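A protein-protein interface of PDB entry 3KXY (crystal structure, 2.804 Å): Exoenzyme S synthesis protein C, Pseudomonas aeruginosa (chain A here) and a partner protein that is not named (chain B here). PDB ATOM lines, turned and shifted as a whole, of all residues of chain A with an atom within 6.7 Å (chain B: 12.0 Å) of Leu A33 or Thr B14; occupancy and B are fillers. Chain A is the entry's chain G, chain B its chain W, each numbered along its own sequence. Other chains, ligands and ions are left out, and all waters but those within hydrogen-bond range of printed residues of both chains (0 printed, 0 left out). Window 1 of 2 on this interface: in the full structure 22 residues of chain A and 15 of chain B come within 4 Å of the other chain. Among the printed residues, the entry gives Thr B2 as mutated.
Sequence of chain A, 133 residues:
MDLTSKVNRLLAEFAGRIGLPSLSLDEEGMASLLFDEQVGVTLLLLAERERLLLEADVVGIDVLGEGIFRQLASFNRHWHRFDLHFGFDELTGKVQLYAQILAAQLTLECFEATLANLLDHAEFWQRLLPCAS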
ATOM      1  N   LEU A  11     -16.179  27.238 -17.793  1.00  0.00           N
ATOM      2  CA  LEU A  11     -17.412  26.501 -17.545  1.00  0.00           C
ATOM      3  C   LEU A  11     -18.425  27.339 -16.767  1.00  0.00           C
ATOM      4  O   LEU A  11     -19.631  27.125 -16.873  1.00  0.00           O
ATOM      5  CB  LEU A  11     -17.116  25.194 -16.808  1.00  0.00           C
ATOM      6  CG  LEU A  11     -16.327  24.154 -17.609  1.00  0.00           C
ATOM      7  CD1 LEU A  11     -15.897  22.994 -16.723  1.00  0.00           C
ATOM      8  CD2 LEU A  11     -17.141  23.656 -18.796  1.00  0.00           C
ATOM      9  N   PHE A  14     -19.862  29.635 -19.449  1.00  0.00           N
ATOM     10  CA  PHE A  14     -20.711  28.806 -20.295  1.00  0.00           C
ATOM     11  C   PHE A  14     -22.044  28.523 -19.613  1.00  0.00           C
ATOM     12  O   PHE A  14     -23.093  28.529 -20.254  1.00  0.00           O
ATOM     13  CB  PHE A  14     -20.008  27.490 -20.627  1.00  0.00           C
ATOM     14  CG  PHE A  14     -20.886  26.491 -21.328  1.00  0.00           C
ATOM     15  CD1 PHE A  14     -21.289  26.698 -22.635  1.00  0.00           C
ATOM     16  CD2 PHE A  14     -21.297  25.337 -20.681  1.00  0.00           C
ATOM     17  CE1 PHE A  14     -22.092  25.778 -23.282  1.00  0.00           C
ATOM     18  CE2 PHE A  14     -22.100  24.411 -21.325  1.00  0.00           C
ATOM     19  CZ  PHE A  14     -22.498  24.633 -22.627  1.00  0.00           C
ATOM     20  N   ILE A  18     -26.200  29.430 -20.795  1.00  0.00           N
ATOM     21  CA  ILE A  18     -27.239  28.445 -21.085  1.00  0.00           C
ATOM     22  C   ILE A  18     -28.341  28.373 -20.027  1.00  0.00           C
ATOM     23  O   ILE A  18     -29.411  27.824 -20.279  1.00  0.00           O
ATOM     24  CB  ILE A  18     -26.643  27.044 -21.307  1.00  0.00           C
ATOM     25  CG1 ILE A  18     -25.980  26.531 -20.027  1.00  0.00           C
ATOM     26  CG2 ILE A  18     -25.651  27.071 -22.457  1.00  0.00           C
ATOM     27  CD1 ILE A  18     -25.435  25.122 -20.149  1.00  0.00           C
ATOM     28  N   LEU A  20     -27.702  27.504 -16.497  1.00  0.00           N
ATOM     29  CA  LEU A  20     -27.384  26.667 -15.348  1.00  0.00           C
ATOM     30  C   LEU A  20     -26.730  27.505 -14.258  1.00  0.00           C
ATOM     31  O   LEU A  20     -25.883  28.351 -14.545  1.00  0.00           O
ATOM     32  CB  LEU A  20     -26.473  25.505 -15.746  1.00  0.00           C
ATOM     33  CG  LEU A  20     -27.090  24.425 -16.635  1.00  0.00           C
ATOM     34  CD1 LEU A  20     -26.110  23.282 -16.831  1.00  0.00           C
ATOM     35  CD2 LEU A  20     -28.389  23.918 -16.031  1.00  0.00           C
ATOM     36  N   LEU A  23     -21.256  25.469 -12.936  1.00  0.00           N
ATOM     37  CA  LEU A  23     -20.649  24.330 -13.613  1.00  0.00           C
ATOM     38  C   LEU A  23     -19.152  24.292 -13.344  1.00  0.00           C
ATOM     39  O   LEU A  23     -18.435  25.250 -13.636  1.00  0.00           O
ATOM     40  CB  LEU A  23     -20.914  24.393 -15.118  1.00  0.00           C
ATOM     41  CG  LEU A  23     -20.393  23.215 -15.942  1.00  0.00           C
ATOM     42  CD1 LEU A  23     -21.002  21.911 -15.451  1.00  0.00           C
ATOM     43  CD2 LEU A  23     -20.686  23.424 -17.420  1.00  0.00           C
ATOM     44  N   ALA A  31     -16.977  16.503 -15.413  1.00  0.00           N
ATOM     45  CA  ALA A  31     -18.293  17.128 -15.324  1.00  0.00           C
ATOM     46  C   ALA A  31     -19.184  16.586 -16.433  1.00  0.00           C
ATOM     47  O   ALA A  31     -18.773  16.529 -17.590  1.00  0.00           O
ATOM     48  CB  ALA A  31     -18.172  18.638 -15.425  1.00  0.00           C
ATOM     49  N   SER A  32     -20.400  16.185 -16.081  1.00  0.00           N
ATOM     50  CA  SER A  32     -21.302  15.580 -17.055  1.00  0.00           C
ATOM     51  C   SER A  32     -22.583  16.381 -17.253  1.00  0.00           C
ATOM     52  O   SER A  32     -23.070  17.037 -16.333  1.00  0.00           O
ATOM     53  CB  SER A  32     -21.632  14.138 -16.662  1.00  0.00           C
ATOM     54  OG  SER A  32     -20.475  13.321 -16.703  1.00  0.00           O
ATOM     55  N   LEU A  33     -23.118  16.317 -18.469  1.00  0.00           N
ATOM     56  CA  LEU A  33     -24.346  17.012 -18.825  1.00  0.00           C
ATOM     57  C   LEU A  33     -25.292  16.062 -19.549  1.00  0.00           C
ATOM     58  O   LEU A  33     -24.876  15.006 -20.024  1.00  0.00           O
ATOM     59  CB  LEU A  33     -24.035  18.213 -19.719  1.00  0.00           C
ATOM     60  CG  LEU A  33     -23.109  19.283 -19.137  1.00  0.00           C
ATOM     61  CD1 LEU A  33     -22.577  20.193 -20.235  1.00  0.00           C
ATOM     62  CD2 LEU A  33     -23.823  20.085 -18.062  1.00  0.00           C
ATOM     63  N   LEU A  34     -26.562  16.440 -19.634  1.00  0.00           N
ATOM     64  CA  LEU A  34     -27.556  15.627 -20.328  1.00  0.00           C
ATOM     65  C   LEU A  34     -28.432  16.484 -21.238  1.00  0.00           C
ATOM     66  O   LEU A  34     -29.206  17.315 -20.765  1.00  0.00           O
ATOM     67  CB  LEU A  34     -28.421  14.864 -19.323  1.00  0.00           C
ATOM     68  CG  LEU A  34     -29.460  13.919 -19.927  1.00  0.00           C
ATOM     69  CD1 LEU A  34     -28.797  12.942 -20.886  1.00  0.00           C
ATOM     70  CD2 LEU A  34     -30.215  13.182 -18.833  1.00  0.00           C
ATOM     71  N   PHE A  35     -28.303  16.272 -22.544  1.00  0.00           N
ATOM     72  CA  PHE A  35     -29.016  17.078 -23.532  1.00  0.00           C
ATOM     73  C   PHE A  35     -30.282  16.390 -24.031  1.00  0.00           C
ATOM     74  O   PHE A  35     -30.242  15.242 -24.474  1.00  0.00           O
ATOM     75  CB  PHE A  35     -28.100  17.403 -24.713  1.00  0.00           C
ATOM     76  CG  PHE A  35     -26.866  18.164 -24.327  1.00  0.00           C
ATOM     77  CD1 PHE A  35     -26.866  19.547 -24.319  1.00  0.00           C
ATOM     78  CD2 PHE A  35     -25.709  17.497 -23.965  1.00  0.00           C
ATOM     79  CE1 PHE A  35     -25.736  20.252 -23.961  1.00  0.00           C
ATOM     80  CE2 PHE A  35     -24.576  18.195 -23.605  1.00  0.00           C
ATOM     81  CZ  PHE A  35     -24.588  19.575 -23.603  1.00  0.00           C
ATOM     82  N   ASP A  36     -31.401  17.105 -23.961  1.00  0.00           N
ATOM     83  CA  ASP A  36     -32.691  16.573 -24.390  1.00  0.00           C
ATOM     84  C   ASP A  36     -33.022  15.241 -23.722  1.00  0.00           C
ATOM     85  O   ASP A  36     -33.783  14.438 -24.263  1.00  0.00           O
ATOM     86  CB  ASP A  36     -32.741  16.430 -25.914  1.00  0.00           C
ATOM     87  CG  ASP A  36     -33.017  17.747 -26.614  1.00  0.00           C
ATOM     88  OD1 ASP A  36     -33.494  18.690 -25.947  1.00  0.00           O
ATOM     89  OD2 ASP A  36     -32.765  17.837 -27.835  1.00  0.00           O
ATOM     90  N   GLU A  37     -32.444  15.015 -22.546  1.00  0.00           N
ATOM     91  CA  GLU A  37     -32.705  13.808 -21.768  1.00  0.00           C
ATOM     92  C   GLU A  37     -32.308  12.543 -22.525  1.00  0.00           C
ATOM     93  O   GLU A  37     -32.744  11.446 -22.178  1.00  0.00           O
ATOM     94  CB  GLU A  37     -34.187  13.729 -21.391  1.00  0.00           C
ATOM     95  CG  GLU A  37     -34.767  15.028 -20.856  1.00  0.00           C
ATOM     96  CD  GLU A  37     -36.264  14.941 -20.616  1.00  0.00           C
ATOM     97  OE1 GLU A  37     -36.927  15.999 -20.589  1.00  0.00           O
ATOM     98  OE2 GLU A  37     -36.777  13.813 -20.460  1.00  0.00           O
ATOM     99  N   VAL A  39     -28.938  12.530 -24.910  1.00  0.00           N
ATOM    100  CA  VAL A  39     -27.503  12.493 -25.174  1.00  0.00           C
ATOM    101  C   VAL A  39     -26.683  12.995 -23.990  1.00  0.00           C
ATOM    102  O   VAL A  39     -26.708  14.180 -23.662  1.00  0.00           O
ATOM    103  CB  VAL A  39     -27.137  13.322 -26.417  1.00  0.00           C
ATOM    104  CG1 VAL A  39     -25.644  13.226 -26.692  1.00  0.00           C
ATOM    105  CG2 VAL A  39     -27.937  12.855 -27.621  1.00  0.00           C
ATOM    106  N   GLY A  40     -25.949  12.085 -23.357  1.00  0.00           N
ATOM    107  CA  GLY A  40     -25.096  12.435 -22.236  1.00  0.00           C
ATOM    108  C   GLY A  40     -23.689  12.792 -22.677  1.00  0.00           C
ATOM    109  O   GLY A  40     -23.084  12.092 -23.488  1.00  0.00           O
ATOM    110  N   VAL A  41     -23.167  13.888 -22.139  1.00  0.00           N
ATOM    111  CA  VAL A  41     -21.824  14.344 -22.476  1.00  0.00           C
ATOM    112  C   VAL A  41     -20.988  14.522 -21.212  1.00  0.00           C
ATOM    113  O   VAL A  41     -21.457  15.081 -20.224  1.00  0.00           O
ATOM    114  CB  VAL A  41     -21.860  15.667 -23.270  1.00  0.00           C
ATOM    115  CG1 VAL A  41     -20.453  16.206 -23.488  1.00  0.00           C
ATOM    116  CG2 VAL A  41     -22.575  15.468 -24.599  1.00  0.00           C
ATOM    117  N   THR A  42     -19.751  14.037 -21.246  1.00  0.00           N
ATOM    118  CA  THR A  42     -18.865  14.137 -20.093  1.00  0.00           C
ATOM    119  C   THR A  42     -17.585  14.893 -20.436  1.00  0.00           C
ATOM    120  O   THR A  42     -16.964  14.644 -21.470  1.00  0.00           O
ATOM    121  CB  THR A  42     -18.513  12.746 -19.527  1.00  0.00           C
ATOM    122  OG1 THR A  42     -19.715  12.059 -19.159  1.00  0.00           O
ATOM    123  CG2 THR A  42     -17.617  12.873 -18.303  1.00  0.00           C
ATOM    124  N   LEU A  43     -17.202  15.821 -19.564  1.00  0.00           N
ATOM    125  CA  LEU A  43     -15.991  16.610 -19.756  1.00  0.00           C
ATOM    126  C   LEU A  43     -14.847  16.029 -18.932  1.00  0.00           C
ATOM    127  O   LEU A  43     -15.016  15.724 -17.753  1.00  0.00           O
ATOM    128  CB  LEU A  43     -16.232  18.067 -19.353  1.00  0.00           C
ATOM    129  CG  LEU A  43     -17.534  18.719 -19.825  1.00  0.00           C
ATOM    130  CD1 LEU A  43     -17.637  20.141 -19.297  1.00  0.00           C
ATOM    131  CD2 LEU A  43     -17.644  18.698 -21.340  1.00  0.00           C
ATOM    132  N   PHE A 111     -15.022  26.055 -27.344  1.00  0.00           N
ATOM    133  CA  PHE A 111     -15.661  25.028 -26.528  1.00  0.00           C
ATOM    134  C   PHE A 111     -17.108  24.791 -26.946  1.00  0.00           C
ATOM    135  O   PHE A 111     -17.544  23.647 -27.086  1.00  0.00           O
ATOM    136  CB  PHE A 111     -15.605  25.401 -25.045  1.00  0.00           C
ATOM    137  CG  PHE A 111     -16.420  24.497 -24.162  1.00  0.00           C
ATOM    138  CD1 PHE A 111     -15.932  23.262 -23.774  1.00  0.00           C
ATOM    139  CD2 PHE A 111     -17.674  24.886 -23.718  1.00  0.00           C
ATOM    140  CE1 PHE A 111     -16.680  22.429 -22.964  1.00  0.00           C
ATOM    141  CE2 PHE A 111     -18.426  24.057 -22.906  1.00  0.00           C
ATOM    142  CZ  PHE A 111     -17.929  22.828 -22.530  1.00  0.00           C
ATOM    143  N   LEU A 115     -18.596  21.473 -28.881  1.00  0.00           N
ATOM    144  CA  LEU A 115     -19.682  20.761 -28.224  1.00  0.00           C
ATOM    145  C   LEU A 115     -20.895  20.646 -29.143  1.00  0.00           C
ATOM    146  O   LEU A 115     -21.500  19.579 -29.257  1.00  0.00           O
ATOM    147  CB  LEU A 115     -20.066  21.457 -26.919  1.00  0.00           C
ATOM    148  CG  LEU A 115     -21.143  20.779 -26.072  1.00  0.00           C
ATOM    149  CD1 LEU A 115     -20.708  19.376 -25.676  1.00  0.00           C
ATOM    150  CD2 LEU A 115     -21.461  21.615 -24.841  1.00  0.00           C
ATOM    151  N   THR B   2     -36.633  22.147  -7.172  1.00  0.00           N
ATOM    152  CA  THR B   2     -36.778  22.060  -8.622  1.00  0.00           C
ATOM    153  C   THR B   2     -35.423  21.892  -9.301  1.00  0.00           C
ATOM    154  O   THR B   2     -34.432  22.500  -8.896  1.00  0.00           O
ATOM    155  CB  THR B   2     -37.475  23.309  -9.197  1.00  0.00           C
ATOM    156  OG1 THR B   2     -36.657  24.464  -8.976  1.00  0.00           O
ATOM    157  CG2 THR B   2     -38.832  23.518  -8.537  1.00  0.00           C
ATOM    158  N   GLU B   3     -35.389  21.062 -10.339  1.00  0.00           N
ATOM    159  CA  GLU B   3     -34.161  20.823 -11.088  1.00  0.00           C
ATOM    160  C   GLU B   3     -33.941  21.913 -12.130  1.00  0.00           C
ATOM    161  O   GLU B   3     -34.822  22.197 -12.942  1.00  0.00           O
ATOM    162  CB  GLU B   3     -34.206  19.453 -11.765  1.00  0.00           C
ATOM    163  CG  GLU B   3     -32.933  19.084 -12.513  1.00  0.00           C
ATOM    164  CD  GLU B   3     -33.046  17.759 -13.241  1.00  0.00           C
ATOM    165  OE1 GLU B   3     -34.185  17.318 -13.503  1.00  0.00           O
ATOM    166  OE2 GLU B   3     -31.996  17.156 -13.552  1.00  0.00           O
ATOM    167  N   ALA B   4     -32.760  22.523 -12.104  1.00  0.00           N
ATOM    168  CA  ALA B   4     -32.416  23.562 -13.066  1.00  0.00           C
ATOM    169  C   ALA B   4     -32.289  22.984 -14.469  1.00  0.00           C
ATOM    170  O   ALA B   4     -31.680  21.931 -14.661  1.00  0.00           O
ATOM    171  CB  ALA B   4     -31.125  24.255 -12.656  1.00  0.00           C
ATOM    172  N   VAL B   5     -32.871  23.676 -15.445  1.00  0.00           N
ATOM    173  CA  VAL B   5     -32.796  23.256 -16.840  1.00  0.00           C
ATOM    174  C   VAL B   5     -32.285  24.389 -17.724  1.00  0.00           C
ATOM    175  O   VAL B   5     -32.837  25.488 -17.715  1.00  0.00           O
ATOM    176  CB  VAL B   5     -34.165  22.795 -17.373  1.00  0.00           C
ATOM    177  CG1 VAL B   5     -34.068  22.464 -18.855  1.00  0.00           C
ATOM    178  CG2 VAL B   5     -34.668  21.597 -16.585  1.00  0.00           C
ATOM    179  N   GLY B   6     -31.232  24.113 -18.488  1.00  0.00           N
ATOM    180  CA  GLY B   6     -30.641  25.105 -19.367  1.00  0.00           C
ATOM    181  C   GLY B   6     -30.942  24.848 -20.831  1.00  0.00           C
ATOM    182  O   GLY B   6     -31.606  23.871 -21.173  1.00  0.00           O
ATOM    183  N   HIS B   7     -30.452  25.729 -21.698  1.00  0.00           N
ATOM    184  CA  HIS B   7     -30.701  25.616 -23.131  1.00  0.00           C
ATOM    185  C   HIS B   7     -29.437  25.888 -23.941  1.00  0.00           C
ATOM    186  O   HIS B   7     -28.808  26.938 -23.800  1.00  0.00           O
ATOM    187  CB  HIS B   7     -31.811  26.577 -23.555  1.00  0.00           C
ATOM    188  CG  HIS B   7     -32.220  26.433 -24.988  1.00  0.00           C
ATOM    189  ND1 HIS B   7     -33.258  25.618 -25.386  1.00  0.00           N
ATOM    190  CD2 HIS B   7     -31.733  27.001 -26.116  1.00  0.00           C
ATOM    191  CE1 HIS B   7     -33.392  25.690 -26.699  1.00  0.00           C
ATOM    192  NE2 HIS B   7     -32.478  26.522 -27.166  1.00  0.00           N
ATOM    193  N   PHE B   8     -29.071  24.934 -24.792  1.00  0.00           N
ATOM    194  CA  PHE B   8     -27.886  25.072 -25.630  1.00  0.00           C
ATOM    195  C   PHE B   8     -28.165  24.639 -27.065  1.00  0.00           C
ATOM    196  O   PHE B   8     -28.425  23.464 -27.331  1.00  0.00           O
ATOM    197  CB  PHE B   8     -26.721  24.266 -25.053  1.00  0.00           C
ATOM    198  CG  PHE B   8     -25.461  24.353 -25.868  1.00  0.00           C
ATOM    199  CD1 PHE B   8     -24.607  25.433 -25.731  1.00  0.00           C
ATOM    200  CD2 PHE B   8     -25.133  23.354 -26.769  1.00  0.00           C
ATOM    201  CE1 PHE B   8     -23.450  25.517 -26.480  1.00  0.00           C
ATOM    202  CE2 PHE B   8     -23.975  23.431 -27.521  1.00  0.00           C
ATOM    203  CZ  PHE B   8     -23.134  24.514 -27.377  1.00  0.00           C
ATOM    204  N   GLU B   9     -28.110  25.600 -27.983  1.00  0.00           N
ATOM    205  CA  GLU B   9     -28.313  25.346 -29.406  1.00  0.00           C
ATOM    206  C   GLU B   9     -29.541  24.483 -29.680  1.00  0.00           C
ATOM    207  O   GLU B   9     -29.444  23.440 -30.327  1.00  0.00           O
ATOM    208  CB  GLU B   9     -27.064  24.709 -30.022  1.00  0.00           C
ATOM    209  CG  GLU B   9     -25.806  25.552 -29.869  1.00  0.00           C
ATOM    210  CD  GLU B   9     -25.923  26.909 -30.541  1.00  0.00           C
ATOM    211  OE1 GLU B   9     -26.588  27.001 -31.595  1.00  0.00           O
ATOM    212  OE2 GLU B   9     -25.341  27.884 -30.019  1.00  0.00           O
ATOM    213  N   GLY B  10     -30.692  24.927 -29.186  1.00  0.00           N
ATOM    214  CA  GLY B  10     -31.946  24.233 -29.419  1.00  0.00           C
ATOM    215  C   GLY B  10     -32.051  22.918 -28.674  1.00  0.00           C
ATOM    216  O   GLY B  10     -32.744  21.999 -29.109  1.00  0.00           O
ATOM    217  N   ARG B  11     -31.357  22.825 -27.545  1.00  0.00           N
ATOM    218  CA  ARG B  11     -31.382  21.616 -26.733  1.00  0.00           C
ATOM    219  C   ARG B  11     -31.505  21.950 -25.254  1.00  0.00           C
ATOM    220  O   ARG B  11     -30.853  22.869 -24.760  1.00  0.00           O
ATOM    221  CB  ARG B  11     -30.117  20.786 -26.966  1.00  0.00           C
ATOM    222  CG  ARG B  11     -29.919  20.337 -28.402  1.00  0.00           C
ATOM    223  CD  ARG B  11     -28.641  19.533 -28.556  1.00  0.00           C
ATOM    224  NE  ARG B  11     -28.444  19.090 -29.933  1.00  0.00           N
ATOM    225  CZ  ARG B  11     -27.743  19.762 -30.839  1.00  0.00           C
ATOM    226  NH1 ARG B  11     -27.163  20.910 -30.517  1.00  0.00           N
ATOM    227  NH2 ARG B  11     -27.618  19.283 -32.069  1.00  0.00           N
ATOM    228  N   SER B  12     -32.350  21.204 -24.551  1.00  0.00           N
ATOM    229  CA  SER B  12     -32.456  21.343 -23.106  1.00  0.00           C
ATOM    230  C   SER B  12     -31.228  20.715 -22.456  1.00  0.00           C
ATOM    231  O   SER B  12     -30.665  19.751 -22.979  1.00  0.00           O
ATOM    232  CB  SER B  12     -33.734  20.680 -22.596  1.00  0.00           C
ATOM    233  OG  SER B  12     -33.821  19.339 -23.044  1.00  0.00           O
ATOM    234  N   VAL B  13     -30.808  21.269 -21.324  1.00  0.00           N
ATOM    235  CA  VAL B  13     -29.607  20.795 -20.646  1.00  0.00           C
ATOM    236  C   VAL B  13     -29.807  20.713 -19.137  1.00  0.00           C
ATOM    237  O   VAL B  13     -30.243  21.677 -18.509  1.00  0.00           O
ATOM    238  CB  VAL B  13     -28.403  21.716 -20.925  1.00  0.00           C
ATOM    239  CG1 VAL B  13     -27.128  21.101 -20.371  1.00  0.00           C
ATOM    240  CG2 VAL B  13     -28.265  21.984 -22.415  1.00  0.00           C
ATOM    241  N   THR B  14     -29.484  19.561 -18.559  1.00  0.00           N
ATOM    242  CA  THR B  14     -29.529  19.400 -17.109  1.00  0.00           C
ATOM    243  C   THR B  14     -28.196  18.888 -16.577  1.00  0.00           C
ATOM    244  O   THR B  14     -27.456  18.198 -17.281  1.00  0.00           O
ATOM    245  CB  THR B  14     -30.657  18.444 -16.663  1.00  0.00           C
ATOM    246  OG1 THR B  14     -30.557  17.206 -17.380  1.00  0.00           O
ATOM    247  CG2 THR B  14     -32.018  19.064 -16.925  1.00  0.00           C
ATOM    248  N   ARG B  15     -27.894  19.240 -15.331  1.00  0.00           N
ATOM    249  CA  ARG B  15     -26.680  18.782 -14.670  1.00  0.00           C
ATOM    250  C   ARG B  15     -26.770  17.278 -14.443  1.00  0.00           C
ATOM    251  O   ARG B  15     -27.736  16.792 -13.856  1.00  0.00           O
ATOM    252  CB  ARG B  15     -26.514  19.502 -13.333  1.00  0.00           C
ATOM    253  CG  ARG B  15     -25.132  19.391 -12.712  1.00  0.00           C
ATOM    254  CD  ARG B  15     -24.134  20.291 -13.418  1.00  0.00           C
ATOM    255  NE  ARG B  15     -22.971  20.576 -12.581  1.00  0.00           N
ATOM    256  CZ  ARG B  15     -21.865  19.838 -12.559  1.00  0.00           C
ATOM    257  NH1 ARG B  15     -21.764  18.765 -13.332  1.00  0.00           N
ATOM    258  NH2 ARG B  15     -20.858  20.175 -11.765  1.00  0.00           N
ATOM    259  N   ALA B  16     -25.768  16.542 -14.912  1.00  0.00           N
ATOM    260  CA  ALA B  16     -25.758  15.090 -14.766  1.00  0.00           C
ATOM    261  C   ALA B  16     -24.642  14.626 -13.834  1.00  0.00           C
ATOM    262  O   ALA B  16     -23.606  15.280 -13.716  1.00  0.00           O
ATOM    263  CB  ALA B  16     -25.630  14.419 -16.126  1.00  0.00           C
ATOM    264  N   ALA B  17     -24.863  13.493 -13.173  1.00  0.00           N
ATOM    265  CA  ALA B  17     -23.867  12.930 -12.269  1.00  0.00           C
ATOM    266  C   ALA B  17     -22.723  12.297 -13.054  1.00  0.00           C
ATOM    267  O   ALA B  17     -22.934  11.722 -14.124  1.00  0.00           O
ATOM    268  CB  ALA B  17     -24.505  11.909 -11.339  1.00  0.00           C
ATOM    269  N   VAL B  18     -21.513  12.408 -12.519  1.00  0.00           N
ATOM    270  CA  VAL B  18     -20.331  11.880 -13.187  1.00  0.00           C
ATOM    271  C   VAL B  18     -20.331  10.353 -13.178  1.00  0.00           C
ATOM    272  O   VAL B  18     -19.704   9.719 -14.027  1.00  0.00           O
ATOM    273  CB  VAL B  18     -19.040  12.418 -12.539  1.00  0.00           C
ATOM    274  CG1 VAL B  18     -17.813  11.814 -13.201  1.00  0.00           C
ATOM    275  CG2 VAL B  18     -19.006  13.936 -12.632  1.00  0.00           C
ATOM    276  N   ARG B  19     -21.052   9.773 -12.222  1.00  0.00           N
ATOM    277  CA  ARG B  19     -21.186   8.320 -12.097  1.00  0.00           C
ATOM    278  C   ARG B  19     -19.888   7.555 -12.365  1.00  0.00           C
ATOM    279  O   ARG B  19     -19.890   6.527 -13.041  1.00  0.00           O
ATOM    280  CB  ARG B  19     -22.333   7.795 -12.975  1.00  0.00           C
ATOM    281  CG  ARG B  19     -22.313   8.248 -14.436  1.00  0.00           C
ATOM    282  CD  ARG B  19     -21.439   7.350 -15.302  1.00  0.00           C
ATOM    283  NE  ARG B  19     -21.513   7.703 -16.717  1.00  0.00           N
ATOM    284  CZ  ARG B  19     -20.646   8.498 -17.338  1.00  0.00           C
ATOM    285  NH1 ARG B  19     -19.631   9.026 -16.671  1.00  0.00           N
ATOM    286  NH2 ARG B  19     -20.795   8.761 -18.630  1.00  0.00           N
ATOM    287  N   GLY B  20     -18.786   8.057 -11.817  1.00  0.00           N
ATOM    288  CA  GLY B  20     -17.485   7.440 -12.009  1.00  0.00           C
ATOM    289  C   GLY B  20     -17.424   6.000 -11.530  1.00  0.00           C
ATOM    290  O   GLY B  20     -16.688   5.184 -12.087  1.00  0.00           O
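The side-chain hydroxyl (OG1) of Thr A42 sits at hydrogen-bond distance from the side-chain hydroxyl (OG) of Ser A32, 2.9 Å away. The backbone NH of Leu A33 sits at hydrogen-bond distance from the backbone carbonyl oxygen of Val A41 (2.7 Å). N of Gly B6 sits at hydrogen-bond distance from O of Val B13 (2.6 Å). A ring nitrogen (NE2) of His B7 lies within hydrogen-bond range of the backbone NH (N) of Gly B10 (3.1 Å). NH1 of Arg B11 lies within hydrogen-bond range of O of Glu B9 (3.4 Å).
Of chain B, only Thr B14 and Ala B16 come within 4 Å of Leu A33. Thr B14 touches just these residues of chain A: Leu A33 (3.7 Å) and Leu A34 (3.1 Å). No residue of chain B comes within 4 Å of Ala A31. Ser A32 touches just these residues of chain B: Arg B15, Ala B16, Ala B17 and Val B18. No residue of chain B comes within 4 Å of Glu A37. No residue of chain B comes within 4 Å of Val A41. Thr A42 touches just one residue of chain B: Arg B19 (3.5 Å). Of the printed residues of chain A, Ser B12 touches Leu A34, Phe A35 and Asp A36. Printed residues of chain A within 4 Å of Gly B6: Ile A18 (3.1 Å) and Leu A20 (3.8 Å). Gly B20 touches none of the printed residues of chain A. The nearest residue of chain B that does not touch Leu A33 is Val B13 (4.2 Å). The nearest residue of chain A that does not touch Thr B14 is Ser A32 (4.6 Å). The nearest printed residue of chain B that does not touch Asp A36 is Gly B10 (4.4 Å).
Of the 19 printed residues of chain A, 10 touch a printed residue of chain B. Hydrophobic or aromatic side chains of chain A within 4 Å of the printed part of chain B: Phe A14, Ile A18, Leu A20, Leu A23, Leu A34 and Phe A35. Among the printed residues, 21 pairs touch across the chains. Among the printed residues, no Asp or Glu carboxylate lies within 4 Å of a Lys or Arg side-chain nitrogen of the other chain.
Among the printed residues, merely in contact across the chains: Phe A14 with Phe B8, Ile A18 with Gly B6, Ile A18 with Phe B8, Leu A20 with Gly B6, Leu A20 with Val B13, Leu A23 with Arg B15, Ser A32 with Arg B15, Ser A32 with Ala B17, Ser A32 with Val B18, Leu A33 with Thr B14, Leu A33 with Ala B16, Leu A34 with Ser B12, Leu A34 with Val B13, Phe A35 with Ser B12, Phe A35 with Val B13, Asp A36 with Arg B11 and Thr A42 with Arg B19.
The backbone carbonyl oxygen (O) of Ser B12 lies within hydrogen-bond range of the backbone NH (N) of Asp A36, 2.9 Å away. The backbone carbonyl oxygen (O) of Thr B14 sits at hydrogen-bond distance from the backbone NH (N) of Leu A34 (3.1 Å). The backbone NH of Ala B16 lies within hydrogen-bond range of the backbone carbonyl oxygen of Ser A32, 3.1 Å away. The backbone carbonyl oxygen (O) of Ile A18 lies within hydrogen-bond range of the backbone NH (N) of His B7 (2.7 Å).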
